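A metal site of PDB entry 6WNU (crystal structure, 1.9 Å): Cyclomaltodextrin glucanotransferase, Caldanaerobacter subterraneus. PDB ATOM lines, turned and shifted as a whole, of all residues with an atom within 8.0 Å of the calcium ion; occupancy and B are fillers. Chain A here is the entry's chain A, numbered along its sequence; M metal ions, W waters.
N of Lys 77 lies close to OD1 of Asp 75 (3.5 Å).
OD1 of Asp 48 lies within hydrogen-bond range of OG of Ser 50, at 2.7 Å.
N of Gly 47 sits at hydrogen-bond distance from OD1 of Asp 75, at 2.9 Å.
O of Tyr 45 is in hydrogen-bond range of N of Asp 75, at 3.1 Å.
ND2 of Asn 51 lies close to O of His 131, 3.5 Å away.
The side-chain carboxylate of Asp 75 is in hydrogen-bond range of the backbone NH of Gly 78 (2.8 Å).
The side-chain carboxylate of Asp 48 is in salt-bridge range of the side-chain amino group of Lys 77 (3.6 Å).
The backbone NH (N) of Gly 73 lies within hydrogen-bond range of the side-chain carboxylate (OD1) of Asp 42, 3.0 Å away.
Six residues have an atom within 4 Å of the calcium ion: Asn 46, Asp 48, Asn 51, Asp 52, Gly 73 and Asp 75.
Along chain A the residues within 4 Å of the calcium ion span positions 46 to 75.
OD1 of Asp 52 is bound to the calcium ion (2.3 Å).
OD2 of Asp 75 is bound to the calcium ion, at 2.3 Å.
The calcium ion is bound by OD1 of Asn 51, 2.4 Å away.
The calcium ion is bound by the backbone carbonyl oxygen (O) of Asp 48, 2.4 Å away.
The calcium ion is bound by water W1 (2.5 Å).
The backbone carbonyl oxygen (O) of Gly 73 is bound to the calcium ion (2.5 Å).
The calcium ion is bound by the side-chain amide oxygen (OD1) of Asn 46 (2.6 Å).
The calcium ion has seven donor atoms within binding distance.
Water W1 lies within hydrogen-bond range of O of His 131 (2.7 Å) and O of Asn 51 (3.2 Å).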
ATOM      1  N   VAL A  41     -26.565  10.404  12.755  1.00  0.00           N
ATOM      2  CA  VAL A  41     -25.660   9.323  12.371  1.00  0.00           C
ATOM      3  C   VAL A  41     -24.524   9.152  13.375  1.00  0.00           C
ATOM      4  O   VAL A  41     -24.164   8.028  13.735  1.00  0.00           O
ATOM      5  CB  VAL A  41     -25.113   9.570  10.953  1.00  0.00           C
ATOM      6  CG1 VAL A  41     -23.964   8.637  10.630  1.00  0.00           C
ATOM      7  CG2 VAL A  41     -26.226   9.412   9.954  1.00  0.00           C
ATOM      8  N   ASP A  42     -23.925  10.267  13.817  1.00  0.00           N
ATOM      9  CA  ASP A  42     -22.759  10.200  14.713  1.00  0.00           C
ATOM     10  C   ASP A  42     -23.114   9.595  16.057  1.00  0.00           C
ATOM     11  O   ASP A  42     -22.222   9.120  16.773  1.00  0.00           O
ATOM     12  CB  ASP A  42     -22.172  11.600  14.961  1.00  0.00           C
ATOM     13  CG  ASP A  42     -20.925  11.562  15.857  1.00  0.00           C
ATOM     14  OD1 ASP A  42     -19.908  10.965  15.448  1.00  0.00           O
ATOM     15  OD2 ASP A  42     -20.939  12.140  16.986  1.00  0.00           O
ATOM     16  N   TYR A  45     -24.704   4.470  15.751  1.00  0.00           N
ATOM     17  CA  TYR A  45     -23.905   3.254  15.917  1.00  0.00           C
ATOM     18  C   TYR A  45     -22.561   3.350  15.212  1.00  0.00           C
ATOM     19  O   TYR A  45     -22.518   3.534  13.991  1.00  0.00           O
ATOM     20  CB  TYR A  45     -24.674   2.029  15.413  1.00  0.00           C
ATOM     21  CG  TYR A  45     -24.078   0.720  15.867  1.00  0.00           C
ATOM     22  CD1 TYR A  45     -24.164   0.321  17.206  1.00  0.00           C
ATOM     23  CD2 TYR A  45     -23.426  -0.133  14.980  1.00  0.00           C
ATOM     24  CE1 TYR A  45     -23.615  -0.867  17.648  1.00  0.00           C
ATOM     25  CE2 TYR A  45     -22.887  -1.338  15.412  1.00  0.00           C
ATOM     26  CZ  TYR A  45     -22.990  -1.691  16.739  1.00  0.00           C
ATOM     27  OH  TYR A  45     -22.445  -2.884  17.165  1.00  0.00           O
ATOM     28  N   ASN A  46     -21.477   3.157  15.959  1.00  0.00           N
ATOM     29  CA  ASN A  46     -20.127   3.201  15.416  1.00  0.00           C
ATOM     30  C   ASN A  46     -19.791   1.828  14.837  1.00  0.00           C
ATOM     31  O   ASN A  46     -19.428   0.905  15.572  1.00  0.00           O
ATOM     32  CB  ASN A  46     -19.135   3.595  16.508  1.00  0.00           C
ATOM     33  CG  ASN A  46     -17.718   3.806  15.970  1.00  0.00           C
ATOM     34  OD1 ASN A  46     -17.425   3.533  14.817  1.00  0.00           O
ATOM     35  ND2 ASN A  46     -16.839   4.289  16.825  1.00  0.00           N
ATOM     36  N   GLY A  47     -19.925   1.679  13.530  1.00  0.00           N
ATOM     37  CA  GLY A  47     -19.596   0.434  12.868  1.00  0.00           C
ATOM     38  C   GLY A  47     -18.147   0.274  12.454  1.00  0.00           C
ATOM     39  O   GLY A  47     -17.684  -0.841  12.197  1.00  0.00           O
ATOM     40  N   ASP A  48     -17.398   1.374  12.402  1.00  0.00           N
ATOM     41  CA  ASP A  48     -16.073   1.383  11.765  1.00  0.00           C
ATOM     42  C   ASP A  48     -15.161   2.306  12.542  1.00  0.00           C
ATOM     43  O   ASP A  48     -15.262   3.536  12.423  1.00  0.00           O
ATOM     44  CB  ASP A  48     -16.171   1.818  10.308  1.00  0.00           C
ATOM     45  CG  ASP A  48     -14.845   1.730   9.560  1.00  0.00           C
ATOM     46  OD1 ASP A  48     -13.808   1.445  10.214  1.00  0.00           O
ATOM     47  OD2 ASP A  48     -14.826   1.967   8.334  1.00  0.00           O
ATOM     48  N   PRO A  49     -14.241   1.761  13.338  1.00  0.00           N
ATOM     49  CA  PRO A  49     -13.330   2.626  14.086  1.00  0.00           C
ATOM     50  C   PRO A  49     -12.371   3.406  13.210  1.00  0.00           C
ATOM     51  O   PRO A  49     -11.807   4.400  13.686  1.00  0.00           O
ATOM     52  CB  PRO A  49     -12.571   1.648  14.997  1.00  0.00           C
ATOM     53  CG  PRO A  49     -13.417   0.439  15.044  1.00  0.00           C
ATOM     54  CD  PRO A  49     -14.047   0.350  13.680  1.00  0.00           C
ATOM     55  N   SER A  50     -12.164   2.995  11.953  1.00  0.00           N
ATOM     56  CA  SER A  50     -11.117   3.613  11.137  1.00  0.00           C
ATOM     57  C   SER A  50     -11.495   4.997  10.619  1.00  0.00           C
ATOM     58  O   SER A  50     -10.601   5.734  10.173  1.00  0.00           O
ATOM     59  CB  SER A  50     -10.744   2.699   9.960  1.00  0.00           C
ATOM     60  OG  SER A  50     -11.776   2.662   8.992  1.00  0.00           O
ATOM     61  N   ASN A  51     -12.772   5.371  10.677  1.00  0.00           N
ATOM     62  CA  ASN A  51     -13.190   6.708  10.287  1.00  0.00           C
ATOM     63  C   ASN A  51     -13.563   7.558  11.493  1.00  0.00           C
ATOM     64  O   ASN A  51     -14.200   8.618  11.335  1.00  0.00           O
ATOM     65  CB  ASN A  51     -14.333   6.637   9.258  1.00  0.00           C
ATOM     66  CG  ASN A  51     -15.566   5.918   9.779  1.00  0.00           C
ATOM     67  OD1 ASN A  51     -15.805   5.820  10.975  1.00  0.00           O
ATOM     68  ND2 ASN A  51     -16.366   5.400   8.866  1.00  0.00           N
ATOM     69  N   ASP A  52     -13.179   7.124  12.699  1.00  0.00           N
ATOM     70  CA  ASP A  52     -13.493   7.893  13.906  1.00  0.00           C
ATOM     71  C   ASP A  52     -12.723   9.212  13.934  1.00  0.00           C
ATOM     72  O   ASP A  52     -13.278  10.257  14.290  1.00  0.00           O
ATOM     73  CB  ASP A  52     -13.180   7.066  15.157  1.00  0.00           C
ATOM     74  CG  ASP A  52     -14.184   5.925  15.410  1.00  0.00           C
ATOM     75  OD1 ASP A  52     -15.146   5.737  14.629  1.00  0.00           O
ATOM     76  OD2 ASP A  52     -13.992   5.204  16.414  1.00  0.00           O
ATOM     77  N   ASP A  53     -11.446   9.185  13.562  1.00  0.00           N
ATOM     78  CA  ASP A  53     -10.564  10.348  13.686  1.00  0.00           C
ATOM     79  C   ASP A  53      -9.737  10.501  12.419  1.00  0.00           C
ATOM     80  O   ASP A  53      -8.506  10.334  12.437  1.00  0.00           O
ATOM     81  CB  ASP A  53      -9.683  10.194  14.921  1.00  0.00           C
ATOM     82  CG  ASP A  53      -9.215  11.500  15.474  1.00  0.00           C
ATOM     83  OD1 ASP A  53      -9.692  12.566  15.000  1.00  0.00           O
ATOM     84  OD2 ASP A  53      -8.378  11.475  16.396  1.00  0.00           O
ATOM     85  N   PRO A  54     -10.375  10.849  11.304  1.00  0.00           N
ATOM     86  CA  PRO A  54      -9.678  10.841  10.015  1.00  0.00           C
ATOM     87  C   PRO A  54      -8.596  11.905   9.952  1.00  0.00           C
ATOM     88  O   PRO A  54      -8.703  12.977  10.543  1.00  0.00           O
ATOM     89  CB  PRO A  54     -10.805  11.139   9.014  1.00  0.00           C
ATOM     90  CG  PRO A  54     -12.099  10.863   9.777  1.00  0.00           C
ATOM     91  CD  PRO A  54     -11.777  11.283  11.159  1.00  0.00           C
ATOM     92  N   PHE A  61     -12.673  13.962  17.723  1.00  0.00           N
ATOM     93  CA  PHE A  61     -13.303  12.704  18.123  1.00  0.00           C
ATOM     94  C   PHE A  61     -13.043  12.471  19.611  1.00  0.00           C
ATOM     95  O   PHE A  61     -11.908  12.597  20.073  1.00  0.00           O
ATOM     96  CB  PHE A  61     -12.748  11.557  17.260  1.00  0.00           C
ATOM     97  CG  PHE A  61     -13.061  10.182  17.784  1.00  0.00           C
ATOM     98  CD1 PHE A  61     -14.348   9.679  17.756  1.00  0.00           C
ATOM     99  CD2 PHE A  61     -12.042   9.356  18.233  1.00  0.00           C
ATOM    100  CE1 PHE A  61     -14.629   8.390  18.209  1.00  0.00           C
ATOM    101  CE2 PHE A  61     -12.293   8.079  18.687  1.00  0.00           C
ATOM    102  CZ  PHE A  61     -13.598   7.593  18.675  1.00  0.00           C
ATOM    103  N   TRP A  72     -18.624  11.334  18.095  1.00  0.00           N
ATOM    104  CA  TRP A  72     -18.551  10.169  18.955  1.00  0.00           C
ATOM    105  C   TRP A  72     -18.319   8.867  18.200  1.00  0.00           C
ATOM    106  O   TRP A  72     -18.138   7.818  18.826  1.00  0.00           O
ATOM    107  CB  TRP A  72     -19.827  10.078  19.811  1.00  0.00           C
ATOM    108  CG  TRP A  72     -19.809  11.036  20.972  1.00  0.00           C
ATOM    109  CD1 TRP A  72     -18.863  11.989  21.230  1.00  0.00           C
ATOM    110  CD2 TRP A  72     -20.794  11.150  22.020  1.00  0.00           C
ATOM    111  NE1 TRP A  72     -19.176  12.672  22.386  1.00  0.00           N
ATOM    112  CE2 TRP A  72     -20.363  12.178  22.884  1.00  0.00           C
ATOM    113  CE3 TRP A  72     -21.988  10.478  22.324  1.00  0.00           C
ATOM    114  CZ2 TRP A  72     -21.089  12.562  24.027  1.00  0.00           C
ATOM    115  CZ3 TRP A  72     -22.702  10.851  23.456  1.00  0.00           C
ATOM    116  CH2 TRP A  72     -22.252  11.884  24.282  1.00  0.00           C
ATOM    117  N   GLY A  73     -18.317   8.897  16.850  1.00  0.00           N
ATOM    118  CA  GLY A  73     -17.928   7.744  16.051  1.00  0.00           C
ATOM    119  C   GLY A  73     -19.033   7.060  15.257  1.00  0.00           C
ATOM    120  O   GLY A  73     -18.710   6.202  14.427  1.00  0.00           O
ATOM    121  N   GLY A  74     -20.312   7.393  15.476  1.00  0.00           N
ATOM    122  CA  GLY A  74     -21.370   6.760  14.696  1.00  0.00           C
ATOM    123  C   GLY A  74     -21.220   7.038  13.212  1.00  0.00           C
ATOM    124  O   GLY A  74     -20.780   8.123  12.810  1.00  0.00           O
ATOM    125  N   ASP A  75     -21.567   6.056  12.386  1.00  0.00           N
ATOM    126  CA  ASP A  75     -21.203   6.136  10.968  1.00  0.00           C
ATOM    127  C   ASP A  75     -22.171   5.319  10.117  1.00  0.00           C
ATOM    128  O   ASP A  75     -23.090   4.650  10.608  1.00  0.00           O
ATOM    129  CB  ASP A  75     -19.730   5.721  10.766  1.00  0.00           C
ATOM    130  CG  ASP A  75     -19.400   4.343  11.352  1.00  0.00           C
ATOM    131  OD1 ASP A  75     -20.236   3.412  11.233  1.00  0.00           O
ATOM    132  OD2 ASP A  75     -18.267   4.180  11.893  1.00  0.00           O
ATOM    133  N   LEU A  76     -21.949   5.382   8.799  1.00  0.00           N
ATOM    134  CA  LEU A  76     -22.871   4.743   7.866  1.00  0.00           C
ATOM    135  C   LEU A  76     -22.770   3.218   7.932  1.00  0.00           C
ATOM    136  O   LEU A  76     -23.790   2.524   7.808  1.00  0.00           O
ATOM    137  CB  LEU A  76     -22.607   5.257   6.451  1.00  0.00           C
ATOM    138  CG  LEU A  76     -23.062   6.698   6.147  1.00  0.00           C
ATOM    139  CD1 LEU A  76     -22.355   7.238   4.892  1.00  0.00           C
ATOM    140  CD2 LEU A  76     -24.560   6.786   5.974  1.00  0.00           C
ATOM    141  N   LYS A  77     -21.559   2.687   8.105  1.00  0.00           N
ATOM    142  CA  LYS A  77     -21.421   1.243   8.284  1.00  0.00           C
ATOM    143  C   LYS A  77     -22.282   0.773   9.453  1.00  0.00           C
ATOM    144  O   LYS A  77     -23.004  -0.217   9.351  1.00  0.00           O
ATOM    145  CB  LYS A  77     -19.945   0.883   8.516  1.00  0.00           C
ATOM    146  CG  LYS A  77     -19.678  -0.586   8.886  1.00  0.00           C
ATOM    147  CD  LYS A  77     -19.430  -1.464   7.652  1.00  0.00           C
ATOM    148  CE  LYS A  77     -18.493  -0.811   6.638  1.00  0.00           C
ATOM    149  NZ  LYS A  77     -17.106  -0.593   7.141  1.00  0.00           N
ATOM    150  N   GLY A  78     -22.222   1.494  10.580  1.00  0.00           N
ATOM    151  CA  GLY A  78     -22.996   1.082  11.743  1.00  0.00           C
ATOM    152  C   GLY A  78     -24.494   1.176  11.511  1.00  0.00           C
ATOM    153  O   GLY A  78     -25.248   0.242  11.827  1.00  0.00           O
ATOM    154  N   GLU A 130     -16.415  12.251   5.752  1.00  0.00           N
ATOM    155  CA  GLU A 130     -15.444  11.178   5.929  1.00  0.00           C
ATOM    156  C   GLU A 130     -15.511  10.525   7.317  1.00  0.00           C
ATOM    157  O   GLU A 130     -15.092   9.374   7.451  1.00  0.00           O
ATOM    158  CB  GLU A 130     -14.039  11.717   5.624  1.00  0.00           C
ATOM    159  CG  GLU A 130     -13.491  12.703   6.631  1.00  0.00           C
ATOM    160  CD  GLU A 130     -14.068  14.120   6.505  1.00  0.00           C
ATOM    161  OE1 GLU A 130     -14.841  14.393   5.573  1.00  0.00           O
ATOM    162  OE2 GLU A 130     -13.708  14.958   7.349  1.00  0.00           O
ATOM    163  N   HIS A 131     -15.988  11.238   8.347  1.00  0.00           N
ATOM    164  CA  HIS A 131     -16.267  10.557   9.617  1.00  0.00           C
ATOM    165  C   HIS A 131     -17.332   9.483   9.464  1.00  0.00           C
ATOM    166  O   HIS A 131     -17.321   8.486  10.197  1.00  0.00           O
ATOM    167  CB  HIS A 131     -16.721  11.547  10.706  1.00  0.00           C
ATOM    168  CG  HIS A 131     -15.609  12.371  11.296  1.00  0.00           C
ATOM    169  ND1 HIS A 131     -15.020  13.423  10.627  1.00  0.00           N
ATOM    170  CD2 HIS A 131     -14.997  12.299  12.508  1.00  0.00           C
ATOM    171  CE1 HIS A 131     -14.090  13.958  11.393  1.00  0.00           C
ATOM    172  NE2 HIS A 131     -14.059  13.300  12.537  1.00  0.00           N
ATOM    173  N   PHE A 132     -18.252   9.653   8.505  1.00  0.00           N
ATOM    174  CA  PHE A 132     -19.385   8.746   8.342  1.00  0.00           C
ATOM    175  C   PHE A 132     -19.147   7.658   7.325  1.00  0.00           C
ATOM    176  O   PHE A 132     -19.738   6.575   7.450  1.00  0.00           O
ATOM    177  CB  PHE A 132     -20.668   9.520   7.974  1.00  0.00           C
ATOM    178  CG  PHE A 132     -21.101  10.522   9.002  1.00  0.00           C
ATOM    179  CD1 PHE A 132     -20.623  10.438  10.316  1.00  0.00           C
ATOM    180  CD2 PHE A 132     -21.979  11.560   8.675  1.00  0.00           C
ATOM    181  CE1 PHE A 132     -21.005  11.359  11.285  1.00  0.00           C
ATOM    182  CE2 PHE A 132     -22.367  12.487   9.649  1.00  0.00           C
ATOM    183  CZ  PHE A 132     -21.885  12.386  10.949  1.00  0.00           C
ATOM    184  N   GLY A 133     -18.329   7.903   6.305  1.00  0.00           N
ATOM    185  CA  GLY A 133     -18.011   6.861   5.340  1.00  0.00           C
ATOM    186  C   GLY A 133     -17.625   7.455   4.004  1.00  0.00           C
ATOM    187  O   GLY A 133     -17.380   8.655   3.863  1.00  0.00           O
HETATM  188 CA    CA M   1     -16.748   5.340  13.097  1.00  0.00          CA
HETATM  189  O   HOH W   1     -16.983   7.762  12.725  1.00  0.00           O
